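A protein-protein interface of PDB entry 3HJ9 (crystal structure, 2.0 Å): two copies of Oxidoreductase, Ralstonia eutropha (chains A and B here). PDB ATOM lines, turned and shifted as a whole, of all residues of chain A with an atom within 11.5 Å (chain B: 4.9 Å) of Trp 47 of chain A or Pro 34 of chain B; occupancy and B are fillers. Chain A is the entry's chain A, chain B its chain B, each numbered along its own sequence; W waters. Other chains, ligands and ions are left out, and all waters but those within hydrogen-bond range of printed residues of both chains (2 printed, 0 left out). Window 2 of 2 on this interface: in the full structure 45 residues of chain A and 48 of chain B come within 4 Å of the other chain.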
ATOM      1  N   MET A  40       6.678  13.384  34.717  1.00  0.00           N
ATOM      2  CA  MET A  40       7.410  13.539  33.459  1.00  0.00           C
ATOM      3  C   MET A  40       7.416  15.002  33.041  1.00  0.00           C
ATOM      4  O   MET A  40       6.394  15.649  33.192  1.00  0.00           O
ATOM      5  CB  MET A  40       6.782  12.703  32.329  1.00  0.00           C
ATOM      6  CG  MET A  40       7.601  12.695  31.010  1.00  0.00           C
ATOM      7  SD  MET A  40       6.605  11.819  29.583  1.00  0.00           S
ATOM      8  CE  MET A  40       7.026   9.957  30.104  1.00  0.00           C
ATOM      9  N   PRO A  41       8.573  15.526  32.555  1.00  0.00           N
ATOM     10  CA  PRO A  41       8.623  16.904  32.050  1.00  0.00           C
ATOM     11  C   PRO A  41       7.578  17.176  30.963  1.00  0.00           C
ATOM     12  O   PRO A  41       7.334  16.302  30.143  1.00  0.00           O
ATOM     13  CB  PRO A  41      10.017  16.996  31.437  1.00  0.00           C
ATOM     14  CG  PRO A  41      10.857  16.046  32.226  1.00  0.00           C
ATOM     15  CD  PRO A  41       9.921  14.908  32.587  1.00  0.00           C
ATOM     16  N   LEU A  42       6.955  18.363  30.990  1.00  0.00           N
ATOM     17  CA  LEU A  42       5.967  18.799  29.971  1.00  0.00           C
ATOM     18  C   LEU A  42       6.460  18.517  28.561  1.00  0.00           C
ATOM     19  O   LEU A  42       5.702  17.972  27.762  1.00  0.00           O
ATOM     20  CB  LEU A  42       5.685  20.332  30.050  1.00  0.00           C
ATOM     21  CG  LEU A  42       4.783  20.924  28.944  1.00  0.00           C
ATOM     22  CD1 LEU A  42       3.380  20.395  29.087  1.00  0.00           C
ATOM     23  CD2 LEU A  42       4.810  22.440  28.924  1.00  0.00           C
ATOM     24  N   MET A  43       7.705  18.917  28.272  1.00  0.00           N
ATOM     25  CA  MET A  43       8.313  18.703  26.945  1.00  0.00           C
ATOM     26  C   MET A  43       8.256  17.216  26.573  1.00  0.00           C
ATOM     27  O   MET A  43       7.850  16.894  25.457  1.00  0.00           O
ATOM     28  CB  MET A  43       9.727  19.273  26.839  1.00  0.00           C
ATOM     29  CG  MET A  43       9.795  20.815  26.977  1.00  0.00           C
ATOM     30  SD  MET A  43       8.754  21.783  25.638  1.00  0.00           S
ATOM     31  CE  MET A  43       9.968  21.703  24.095  1.00  0.00           C
ATOM     32  N   GLY A  44       8.583  16.322  27.517  1.00  0.00           N
ATOM     33  CA  GLY A  44       8.429  14.876  27.285  1.00  0.00           C
ATOM     34  C   GLY A  44       6.995  14.446  26.949  1.00  0.00           C
ATOM     35  O   GLY A  44       6.778  13.624  26.044  1.00  0.00           O
ATOM     36  N   THR A  45       6.014  14.999  27.667  1.00  0.00           N
ATOM     37  CA  THR A  45       4.632  14.648  27.436  1.00  0.00           C
ATOM     38  C   THR A  45       4.147  15.129  26.063  1.00  0.00           C
ATOM     39  O   THR A  45       3.353  14.436  25.437  1.00  0.00           O
ATOM     40  CB  THR A  45       3.668  15.107  28.540  1.00  0.00           C
ATOM     41  OG1 THR A  45       3.509  16.517  28.482  1.00  0.00           O
ATOM     42  CG2 THR A  45       4.130  14.646  29.940  1.00  0.00           C
ATOM     43  N   LEU A  46       4.618  16.292  25.608  1.00  0.00           N
ATOM     44  CA  LEU A  46       4.272  16.797  24.256  1.00  0.00           C
ATOM     45  C   LEU A  46       4.811  15.854  23.120  1.00  0.00           C
ATOM     46  O   LEU A  46       4.126  15.619  22.105  1.00  0.00           O
ATOM     47  CB  LEU A  46       4.801  18.228  24.069  1.00  0.00           C
ATOM     48  CG  LEU A  46       4.050  19.281  24.899  1.00  0.00           C
ATOM     49  CD1 LEU A  46       4.790  20.602  24.956  1.00  0.00           C
ATOM     50  CD2 LEU A  46       2.620  19.489  24.367  1.00  0.00           C
ATOM     51  N   TRP A  47       6.028  15.333  23.312  1.00  0.00           N
ATOM     52  CA  TRP A  47       6.612  14.373  22.378  1.00  0.00           C
ATOM     53  C   TRP A  47       5.794  13.075  22.294  1.00  0.00           C
ATOM     54  O   TRP A  47       5.667  12.531  21.221  1.00  0.00           O
ATOM     55  CB  TRP A  47       8.074  14.011  22.716  1.00  0.00           C
ATOM     56  CG  TRP A  47       9.051  15.047  22.276  1.00  0.00           C
ATOM     57  CD1 TRP A  47       9.721  15.939  23.062  1.00  0.00           C
ATOM     58  CD2 TRP A  47       9.444  15.326  20.936  1.00  0.00           C
ATOM     59  NE1 TRP A  47      10.521  16.749  22.297  1.00  0.00           N
ATOM     60  CE2 TRP A  47      10.375  16.398  20.983  1.00  0.00           C
ATOM     61  CE3 TRP A  47       9.119  14.766  19.694  1.00  0.00           C
ATOM     62  CZ2 TRP A  47      10.982  16.929  19.833  1.00  0.00           C
ATOM     63  CZ3 TRP A  47       9.723  15.303  18.540  1.00  0.00           C
ATOM     64  CH2 TRP A  47      10.644  16.372  18.625  1.00  0.00           C
ATOM     65  N   LEU A  48       5.251  12.619  23.425  1.00  0.00           N
ATOM     66  CA  LEU A  48       4.527  11.353  23.513  1.00  0.00           C
ATOM     67  C   LEU A  48       3.014  11.485  23.385  1.00  0.00           C
ATOM     68  O   LEU A  48       2.298  10.472  23.426  1.00  0.00           O
ATOM     69  CB  LEU A  48       4.893  10.648  24.839  1.00  0.00           C
ATOM     70  CG  LEU A  48       6.353  10.266  25.075  1.00  0.00           C
ATOM     71  CD1 LEU A  48       6.614   9.761  26.523  1.00  0.00           C
ATOM     72  CD2 LEU A  48       6.771   9.226  24.048  1.00  0.00           C
ATOM     73  N   ARG A  49       2.512  12.709  23.195  1.00  0.00           N
ATOM     74  CA  ARG A  49       1.056  12.972  23.108  1.00  0.00           C
ATOM     75  C   ARG A  49       0.555  12.318  21.806  1.00  0.00           C
ATOM     76  O   ARG A  49       1.094  12.574  20.728  1.00  0.00           O
ATOM     77  CB  ARG A  49       0.789  14.479  23.181  1.00  0.00           C
ATOM     78  CG  ARG A  49      -0.627  14.929  23.646  1.00  0.00           C
ATOM     79  CD  ARG A  49      -1.776  14.504  22.757  1.00  0.00           C
ATOM     80  NE  ARG A  49      -1.502  14.756  21.340  1.00  0.00           N
ATOM     81  CZ  ARG A  49      -2.128  14.185  20.311  1.00  0.00           C
ATOM     82  NH1 ARG A  49      -3.138  13.335  20.485  1.00  0.00           N
ATOM     83  NH2 ARG A  49      -1.738  14.474  19.074  1.00  0.00           N
ATOM     84  N   LYS A  50      -0.388  11.382  21.942  1.00  0.00           N
ATOM     85  CA  LYS A  50      -0.922  10.596  20.821  1.00  0.00           C
ATOM     86  C   LYS A  50      -2.279  10.008  21.176  1.00  0.00           C
ATOM     87  O   LYS A  50      -2.646   9.982  22.349  1.00  0.00           O
ATOM     88  CB  LYS A  50       0.026   9.429  20.477  1.00  0.00           C
ATOM     89  CG  LYS A  50       0.157   8.340  21.585  1.00  0.00           C
ATOM     90  CD  LYS A  50       1.057   7.173  21.213  1.00  0.00           C
ATOM     91  CE  LYS A  50       0.488   6.333  20.064  1.00  0.00           C
ATOM     92  NZ  LYS A  50       1.331   5.094  19.803  1.00  0.00           N
ATOM     93  N   SER A  51      -2.973   9.470  20.174  1.00  0.00           N
ATOM     94  CA  SER A  51      -4.255   8.793  20.375  1.00  0.00           C
ATOM     95  C   SER A  51      -4.094   7.264  20.377  1.00  0.00           C
ATOM     96  O   SER A  51      -3.380   6.705  19.576  1.00  0.00           O
ATOM     97  CB  SER A  51      -5.308   9.255  19.365  1.00  0.00           C
ATOM     98  OG  SER A  51      -5.660  10.598  19.635  1.00  0.00           O
ATOM     99  N   THR A  52      -4.799   6.611  21.285  1.00  0.00           N
ATOM    100  CA  THR A  52      -4.802   5.153  21.443  1.00  0.00           C
ATOM    101  C   THR A  52      -6.242   4.705  21.354  1.00  0.00           C
ATOM    102  O   THR A  52      -7.118   5.374  21.920  1.00  0.00           O
ATOM    103  CB  THR A  52      -4.240   4.774  22.830  1.00  0.00           C
ATOM    104  OG1 THR A  52      -2.963   5.399  22.974  1.00  0.00           O
ATOM    105  CG2 THR A  52      -4.095   3.215  22.978  1.00  0.00           C
ATOM    106  N   GLU A 169      -7.060  18.120  26.426  1.00  0.00           N
ATOM    107  CA  GLU A 169      -5.610  18.153  26.151  1.00  0.00           C
ATOM    108  C   GLU A 169      -4.790  17.935  27.428  1.00  0.00           C
ATOM    109  O   GLU A 169      -3.783  17.226  27.403  1.00  0.00           O
ATOM    110  CB  GLU A 169      -5.190  19.437  25.426  1.00  0.00           C
ATOM    111  CG  GLU A 169      -3.752  19.458  24.958  1.00  0.00           C
ATOM    112  CD  GLU A 169      -3.394  18.381  23.932  1.00  0.00           C
ATOM    113  OE1 GLU A 169      -4.283  17.606  23.502  1.00  0.00           O
ATOM    114  OE2 GLU A 169      -2.193  18.322  23.543  1.00  0.00           O
ATOM    115  N   TYR A 172      -4.902  14.194  27.909  1.00  0.00           N
ATOM    116  CA  TYR A 172      -3.929  13.567  26.979  1.00  0.00           C
ATOM    117  C   TYR A 172      -2.497  13.591  27.481  1.00  0.00           C
ATOM    118  O   TYR A 172      -1.811  12.566  27.477  1.00  0.00           O
ATOM    119  CB  TYR A 172      -3.931  14.254  25.616  1.00  0.00           C
ATOM    120  CG  TYR A 172      -4.771  13.660  24.524  1.00  0.00           C
ATOM    121  CD1 TYR A 172      -4.449  12.426  23.960  1.00  0.00           C
ATOM    122  CD2 TYR A 172      -5.830  14.390  23.956  1.00  0.00           C
ATOM    123  CE1 TYR A 172      -5.217  11.901  22.855  1.00  0.00           C
ATOM    124  CE2 TYR A 172      -6.566  13.880  22.864  1.00  0.00           C
ATOM    125  CZ  TYR A 172      -6.271  12.664  22.328  1.00  0.00           C
ATOM    126  OH  TYR A 172      -7.021  12.227  21.260  1.00  0.00           O
ATOM    127  N   LEU A 173      -2.068  14.784  27.892  1.00  0.00           N
ATOM    128  CA  LEU A 173      -0.725  15.027  28.415  1.00  0.00           C
ATOM    129  C   LEU A 173      -0.494  14.245  29.717  1.00  0.00           C
ATOM    130  O   LEU A 173       0.572  13.609  29.879  1.00  0.00           O
ATOM    131  CB  LEU A 173      -0.436  16.544  28.576  1.00  0.00           C
ATOM    132  CG  LEU A 173      -0.365  17.337  27.251  1.00  0.00           C
ATOM    133  CD1 LEU A 173      -0.333  18.852  27.477  1.00  0.00           C
ATOM    134  CD2 LEU A 173       0.811  16.877  26.350  1.00  0.00           C
ATOM    135  N   TYR A 174      -1.500  14.230  30.603  1.00  0.00           N
ATOM    136  CA  TYR A 174      -1.416  13.403  31.820  1.00  0.00           C
ATOM    137  C   TYR A 174      -1.243  11.918  31.428  1.00  0.00           C
ATOM    138  O   TYR A 174      -0.343  11.239  31.946  1.00  0.00           O
ATOM    139  CB  TYR A 174      -2.592  13.620  32.798  1.00  0.00           C
ATOM    140  CG  TYR A 174      -2.443  12.697  33.941  1.00  0.00           C
ATOM    141  CD1 TYR A 174      -1.561  12.986  34.987  1.00  0.00           C
ATOM    142  CD2 TYR A 174      -3.072  11.449  33.926  1.00  0.00           C
ATOM    143  CE1 TYR A 174      -1.354  12.056  36.023  1.00  0.00           C
ATOM    144  CE2 TYR A 174      -2.865  10.515  34.954  1.00  0.00           C
ATOM    145  CZ  TYR A 174      -2.027  10.829  35.996  1.00  0.00           C
ATOM    146  OH  TYR A 174      -1.835   9.882  36.975  1.00  0.00           O
ATOM    147  N   CYS A 175      -2.044  11.447  30.479  1.00  0.00           N
ATOM    148  CA  CYS A 175      -1.956  10.048  30.042  1.00  0.00           C
ATOM    149  C   CYS A 175      -0.560   9.691  29.536  1.00  0.00           C
ATOM    150  O   CYS A 175      -0.009   8.631  29.913  1.00  0.00           O
ATOM    151  CB  CYS A 175      -3.043   9.711  29.025  1.00  0.00           C
ATOM    152  SG  CYS A 175      -4.651   9.670  29.835  1.00  0.00           S
ATOM    153  N   ALA A 176       0.028  10.612  28.770  1.00  0.00           N
ATOM    154  CA  ALA A 176       1.392  10.466  28.250  1.00  0.00           C
ATOM    155  C   ALA A 176       2.397  10.420  29.401  1.00  0.00           C
ATOM    156  O   ALA A 176       3.298   9.589  29.375  1.00  0.00           O
ATOM    157  CB  ALA A 176       1.748  11.594  27.258  1.00  0.00           C
ATOM    158  N   SER A 177       2.246  11.305  30.398  1.00  0.00           N
ATOM    159  CA  SER A 177       3.145  11.288  31.578  1.00  0.00           C
ATOM    160  C   SER A 177       3.065   9.991  32.382  1.00  0.00           C
ATOM    161  O   SER A 177       4.055   9.578  32.917  1.00  0.00           O
ATOM    162  CB  SER A 177       2.852  12.428  32.565  1.00  0.00           C
ATOM    163  OG  SER A 177       1.664  12.181  33.329  1.00  0.00           O
ATOM    164  N   LEU A 180      -0.449   5.918  30.013  1.00  0.00           N
ATOM    165  CA  LEU A 180      -1.814   5.539  29.689  1.00  0.00           C
ATOM    166  C   LEU A 180      -2.146   5.989  28.258  1.00  0.00           C
ATOM    167  O   LEU A 180      -1.552   6.930  27.730  1.00  0.00           O
ATOM    168  CB  LEU A 180      -2.797   6.208  30.659  1.00  0.00           C
ATOM    169  CG  LEU A 180      -2.809   5.814  32.137  1.00  0.00           C
ATOM    170  CD1 LEU A 180      -3.767   6.721  32.933  1.00  0.00           C
ATOM    171  CD2 LEU A 180      -3.217   4.327  32.278  1.00  0.00           C
ATOM    172  N   PRO B  32      15.052  26.944  15.204  1.00  0.00           N
ATOM    173  CA  PRO B  32      15.913  25.820  15.615  1.00  0.00           C
ATOM    174  C   PRO B  32      15.076  24.550  15.843  1.00  0.00           C
ATOM    175  O   PRO B  32      13.908  24.642  16.255  1.00  0.00           O
ATOM    176  CB  PRO B  32      16.574  26.330  16.900  1.00  0.00           C
ATOM    177  CG  PRO B  32      15.657  27.353  17.413  1.00  0.00           C
ATOM    178  CD  PRO B  32      15.128  28.041  16.187  1.00  0.00           C
ATOM    179  N   GLU B  33      15.655  23.394  15.519  1.00  0.00           N
ATOM    180  CA  GLU B  33      14.916  22.126  15.556  1.00  0.00           C
ATOM    181  C   GLU B  33      14.459  21.826  16.976  1.00  0.00           C
ATOM    182  O   GLU B  33      15.211  22.054  17.912  1.00  0.00           O
ATOM    183  CB  GLU B  33      15.676  20.919  14.933  1.00  0.00           C
ATOM    184  CG  GLU B  33      16.916  20.439  15.675  1.00  0.00           C
ATOM    185  CD  GLU B  33      17.692  19.266  14.975  1.00  0.00           C
ATOM    186  OE1 GLU B  33      17.190  18.658  13.991  1.00  0.00           O
ATOM    187  OE2 GLU B  33      18.814  18.947  15.437  1.00  0.00           O
ATOM    188  N   PRO B  34      13.197  21.381  17.134  1.00  0.00           N
ATOM    189  CA  PRO B  34      12.735  21.003  18.453  1.00  0.00           C
ATOM    190  C   PRO B  34      13.487  19.726  18.883  1.00  0.00           C
ATOM    191  O   PRO B  34      13.499  18.741  18.128  1.00  0.00           O
ATOM    192  CB  PRO B  34      11.242  20.731  18.243  1.00  0.00           C
ATOM    193  CG  PRO B  34      11.105  20.399  16.791  1.00  0.00           C
ATOM    194  CD  PRO B  34      12.284  20.913  16.070  1.00  0.00           C
ATOM    195  N   ASP B  35      14.186  19.801  20.016  1.00  0.00           N
ATOM    196  CA  ASP B  35      14.915  18.653  20.582  1.00  0.00           C
ATOM    197  C   ASP B  35      14.810  18.447  22.112  1.00  0.00           C
ATOM    198  O   ASP B  35      15.261  17.412  22.605  1.00  0.00           O
ATOM    199  CB  ASP B  35      16.395  18.696  20.143  1.00  0.00           C
ATOM    200  CG  ASP B  35      17.116  19.989  20.543  1.00  0.00           C
ATOM    201  OD1 ASP B  35      16.643  20.754  21.422  1.00  0.00           O
ATOM    202  OD2 ASP B  35      18.187  20.229  19.949  1.00  0.00           O
ATOM    203  N   ARG B  36      14.218  19.388  22.852  1.00  0.00           N
ATOM    204  CA  ARG B  36      14.149  19.262  24.305  1.00  0.00           C
ATOM    205  C   ARG B  36      13.122  18.254  24.810  1.00  0.00           C
ATOM    206  O   ARG B  36      11.984  18.244  24.335  1.00  0.00           O
ATOM    207  CB  ARG B  36      13.848  20.602  24.994  1.00  0.00           C
ATOM    208  CG  ARG B  36      15.066  21.368  25.525  1.00  0.00           C
ATOM    209  CD  ARG B  36      14.671  22.049  26.847  1.00  0.00           C
ATOM    210  NE  ARG B  36      13.524  22.949  26.666  1.00  0.00           N
ATOM    211  CZ  ARG B  36      12.646  23.307  27.607  1.00  0.00           C
ATOM    212  NH1 ARG B  36      12.704  22.809  28.846  1.00  0.00           N
ATOM    213  NH2 ARG B  36      11.651  24.147  27.299  1.00  0.00           N
ATOM    214  N   THR B  37      13.551  17.426  25.762  1.00  0.00           N
ATOM    215  CA  THR B  37      12.666  16.530  26.497  1.00  0.00           C
ATOM    216  C   THR B  37      12.639  16.855  28.011  1.00  0.00           C
ATOM    217  O   THR B  37      11.889  16.215  28.740  1.00  0.00           O
ATOM    218  CB  THR B  37      13.067  15.074  26.324  1.00  0.00           C
ATOM    219  OG1 THR B  37      14.348  14.856  26.943  1.00  0.00           O
ATOM    220  CG2 THR B  37      13.094  14.693  24.834  1.00  0.00           C
ATOM    221  N   TRP B  70       6.163  24.885  18.467  1.00  0.00           N
ATOM    222  CA  TRP B  70       6.220  23.437  18.410  1.00  0.00           C
ATOM    223  C   TRP B  70       5.223  22.841  19.417  1.00  0.00           C
ATOM    224  O   TRP B  70       4.543  21.888  19.101  1.00  0.00           O
ATOM    225  CB  TRP B  70       7.658  22.911  18.638  1.00  0.00           C
ATOM    226  CG  TRP B  70       7.710  21.405  18.669  1.00  0.00           C
ATOM    227  CD1 TRP B  70       7.794  20.560  17.609  1.00  0.00           C
ATOM    228  CD2 TRP B  70       7.606  20.587  19.835  1.00  0.00           C
ATOM    229  NE1 TRP B  70       7.750  19.257  18.045  1.00  0.00           N
ATOM    230  CE2 TRP B  70       7.659  19.246  19.411  1.00  0.00           C
ATOM    231  CE3 TRP B  70       7.463  20.866  21.201  1.00  0.00           C
ATOM    232  CZ2 TRP B  70       7.594  18.170  20.305  1.00  0.00           C
ATOM    233  CZ3 TRP B  70       7.413  19.808  22.094  1.00  0.00           C
ATOM    234  CH2 TRP B  70       7.463  18.461  21.635  1.00  0.00           C
ATOM    235  N   VAL B  75       5.238  18.992  14.903  1.00  0.00           N
ATOM    236  CA  VAL B  75       5.298  17.583  14.577  1.00  0.00           C
ATOM    237  C   VAL B  75       6.094  16.921  15.716  1.00  0.00           C
ATOM    238  O   VAL B  75       7.226  17.327  15.997  1.00  0.00           O
ATOM    239  CB  VAL B  75       5.976  17.352  13.214  1.00  0.00           C
ATOM    240  CG1 VAL B  75       6.234  15.872  12.963  1.00  0.00           C
ATOM    241  CG2 VAL B  75       5.091  17.975  12.096  1.00  0.00           C
ATOM    242  N   ASN B  76       5.465  15.972  16.412  1.00  0.00           N
ATOM    243  CA  ASN B  76       6.147  15.156  17.433  1.00  0.00           C
ATOM    244  C   ASN B  76       6.488  13.754  16.898  1.00  0.00           C
ATOM    245  O   ASN B  76       7.188  13.020  17.566  1.00  0.00           O
ATOM    246  CB  ASN B  76       5.370  15.095  18.764  1.00  0.00           C
ATOM    247  CG  ASN B  76       3.975  14.428  18.647  1.00  0.00           C
ATOM    248  OD1 ASN B  76       3.555  13.989  17.559  1.00  0.00           O
ATOM    249  ND2 ASN B  76       3.258  14.364  19.787  1.00  0.00           N
ATOM    250  N   HIS B 112       8.874  23.378  10.114  1.00  0.00           N
ATOM    251  CA  HIS B 112       9.183  24.084  11.363  1.00  0.00           C
ATOM    252  C   HIS B 112       9.777  25.499  11.098  1.00  0.00           C
ATOM    253  O   HIS B 112      10.952  25.792  11.368  1.00  0.00           O
ATOM    254  CB  HIS B 112      10.082  23.202  12.238  1.00  0.00           C
ATOM    255  CG  HIS B 112      10.306  23.773  13.588  1.00  0.00           C
ATOM    256  ND1 HIS B 112       9.262  24.092  14.428  1.00  0.00           N
ATOM    257  CD2 HIS B 112      11.439  24.127  14.231  1.00  0.00           C
ATOM    258  CE1 HIS B 112       9.750  24.602  15.544  1.00  0.00           C
ATOM    259  NE2 HIS B 112      11.066  24.630  15.450  1.00  0.00           N
HETATM  260  O   HOH W   1       3.683  11.200  20.031  1.00  0.00           O
HETATM  261  O   HOH W   2       7.555  11.123  19.773  1.00  0.00           O
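The side-chain amide nitrogen of Asn 76 of chain B lies within hydrogen-bond range of the backbone carbonyl oxygen of Leu 46 of chain A.
O of Arg 36 of chain B lies within hydrogen-bond range of NE1 of Trp 47 of chain A (2.9 Å).
ND2 of Asn 76 of chain B lies within hydrogen-bond range of O of Arg 49 of chain A.
ND2 of Asn 76 of chain B is in hydrogen-bond range of O of Trp 47 of chain A (3.3 Å).
O of Val 75 of chain B sits at hydrogen-bond distance from NE1 of Trp 70 of chain B (2.9 Å).
Among the printed residues, pairs that only touch across the chains: Trp 47 of chain A with Trp 70 of chain B, Pro 41 of chain A with Thr 37 of chain B, Met 43 of chain A with Arg 36 of chain B, Gly 44 of chain A with Thr 37 of chain B, Trp 47 of chain A with Pro 34 of chain B, Leu 46 of chain A with Trp 70 of chain B, Met 43 of chain A with Trp 70 of chain B and Met 43 of chain A with Thr 37 of chain B.
Printed residues of chain B within 4 Å of Trp 47 of chain A: Pro 34 (3.5 Å), Arg 36 (2.9 Å), Trp 70 (3.4 Å) and Asn 76 (3.3 Å).
Of the printed residues of chain A, Pro 34 of chain B touches Trp 47.
No residue of chain A comes within 4 Å of Glu 33 of chain B.
No residue of chain A comes within 4 Å of Asp 35 of chain B.
Of the printed residues of chain A, Trp 70 of chain B touches Met 43, Leu 46 and Trp 47.
Asn 76 of chain B touches just these residues of chain A: Leu 46, Trp 47 and Arg 49.
No residue of chain A comes within 4 Å of His 112 of chain B.
Of the printed residues of chain B, Gly 44 of chain A touches Thr 37.
Of the printed residues of chain B, Leu 46 of chain A touches Trp 70 and Asn 76.
Of the printed residues of chain B, Arg 49 of chain A touches Asn 76.
Printed residues of chain A within 4 Å of Thr 37 of chain B: Pro 41, Met 43 and Gly 44.
The nearest printed residue of chain B that does not touch Met 43 of chain A is Pro 34 of chain B (6.1 Å).
Of the 21 printed residues of chain A, 6 touch a printed residue of chain B.
Hydrophobic or aromatic side chains of chain A that line the printed part of chain B: Pro 41, Met 43, Leu 46 and Trp 47.
Along chain A the printed residues that touch a printed residue of chain B span positions 41 to 49.
Of the 10 printed residues of chain B, 5 touch a printed residue of chain A.
No position is printed for both chains.
Water W1 lies within hydrogen-bond range of the backbone carbonyl oxygen (O) of Trp 47 of chain A (2.7 Å), the backbone carbonyl oxygen (O) of Arg 49 of chain A (3.0 Å) and the side-chain amide nitrogen (ND2) of Asn 76 of chain B (3.2 Å).
Water W2 bridges the backbone carbonyl oxygen (O) of Trp 47 of chain A (2.8 Å) and the backbone carbonyl oxygen (O) of Asn 76 of chain B (2.9 Å).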
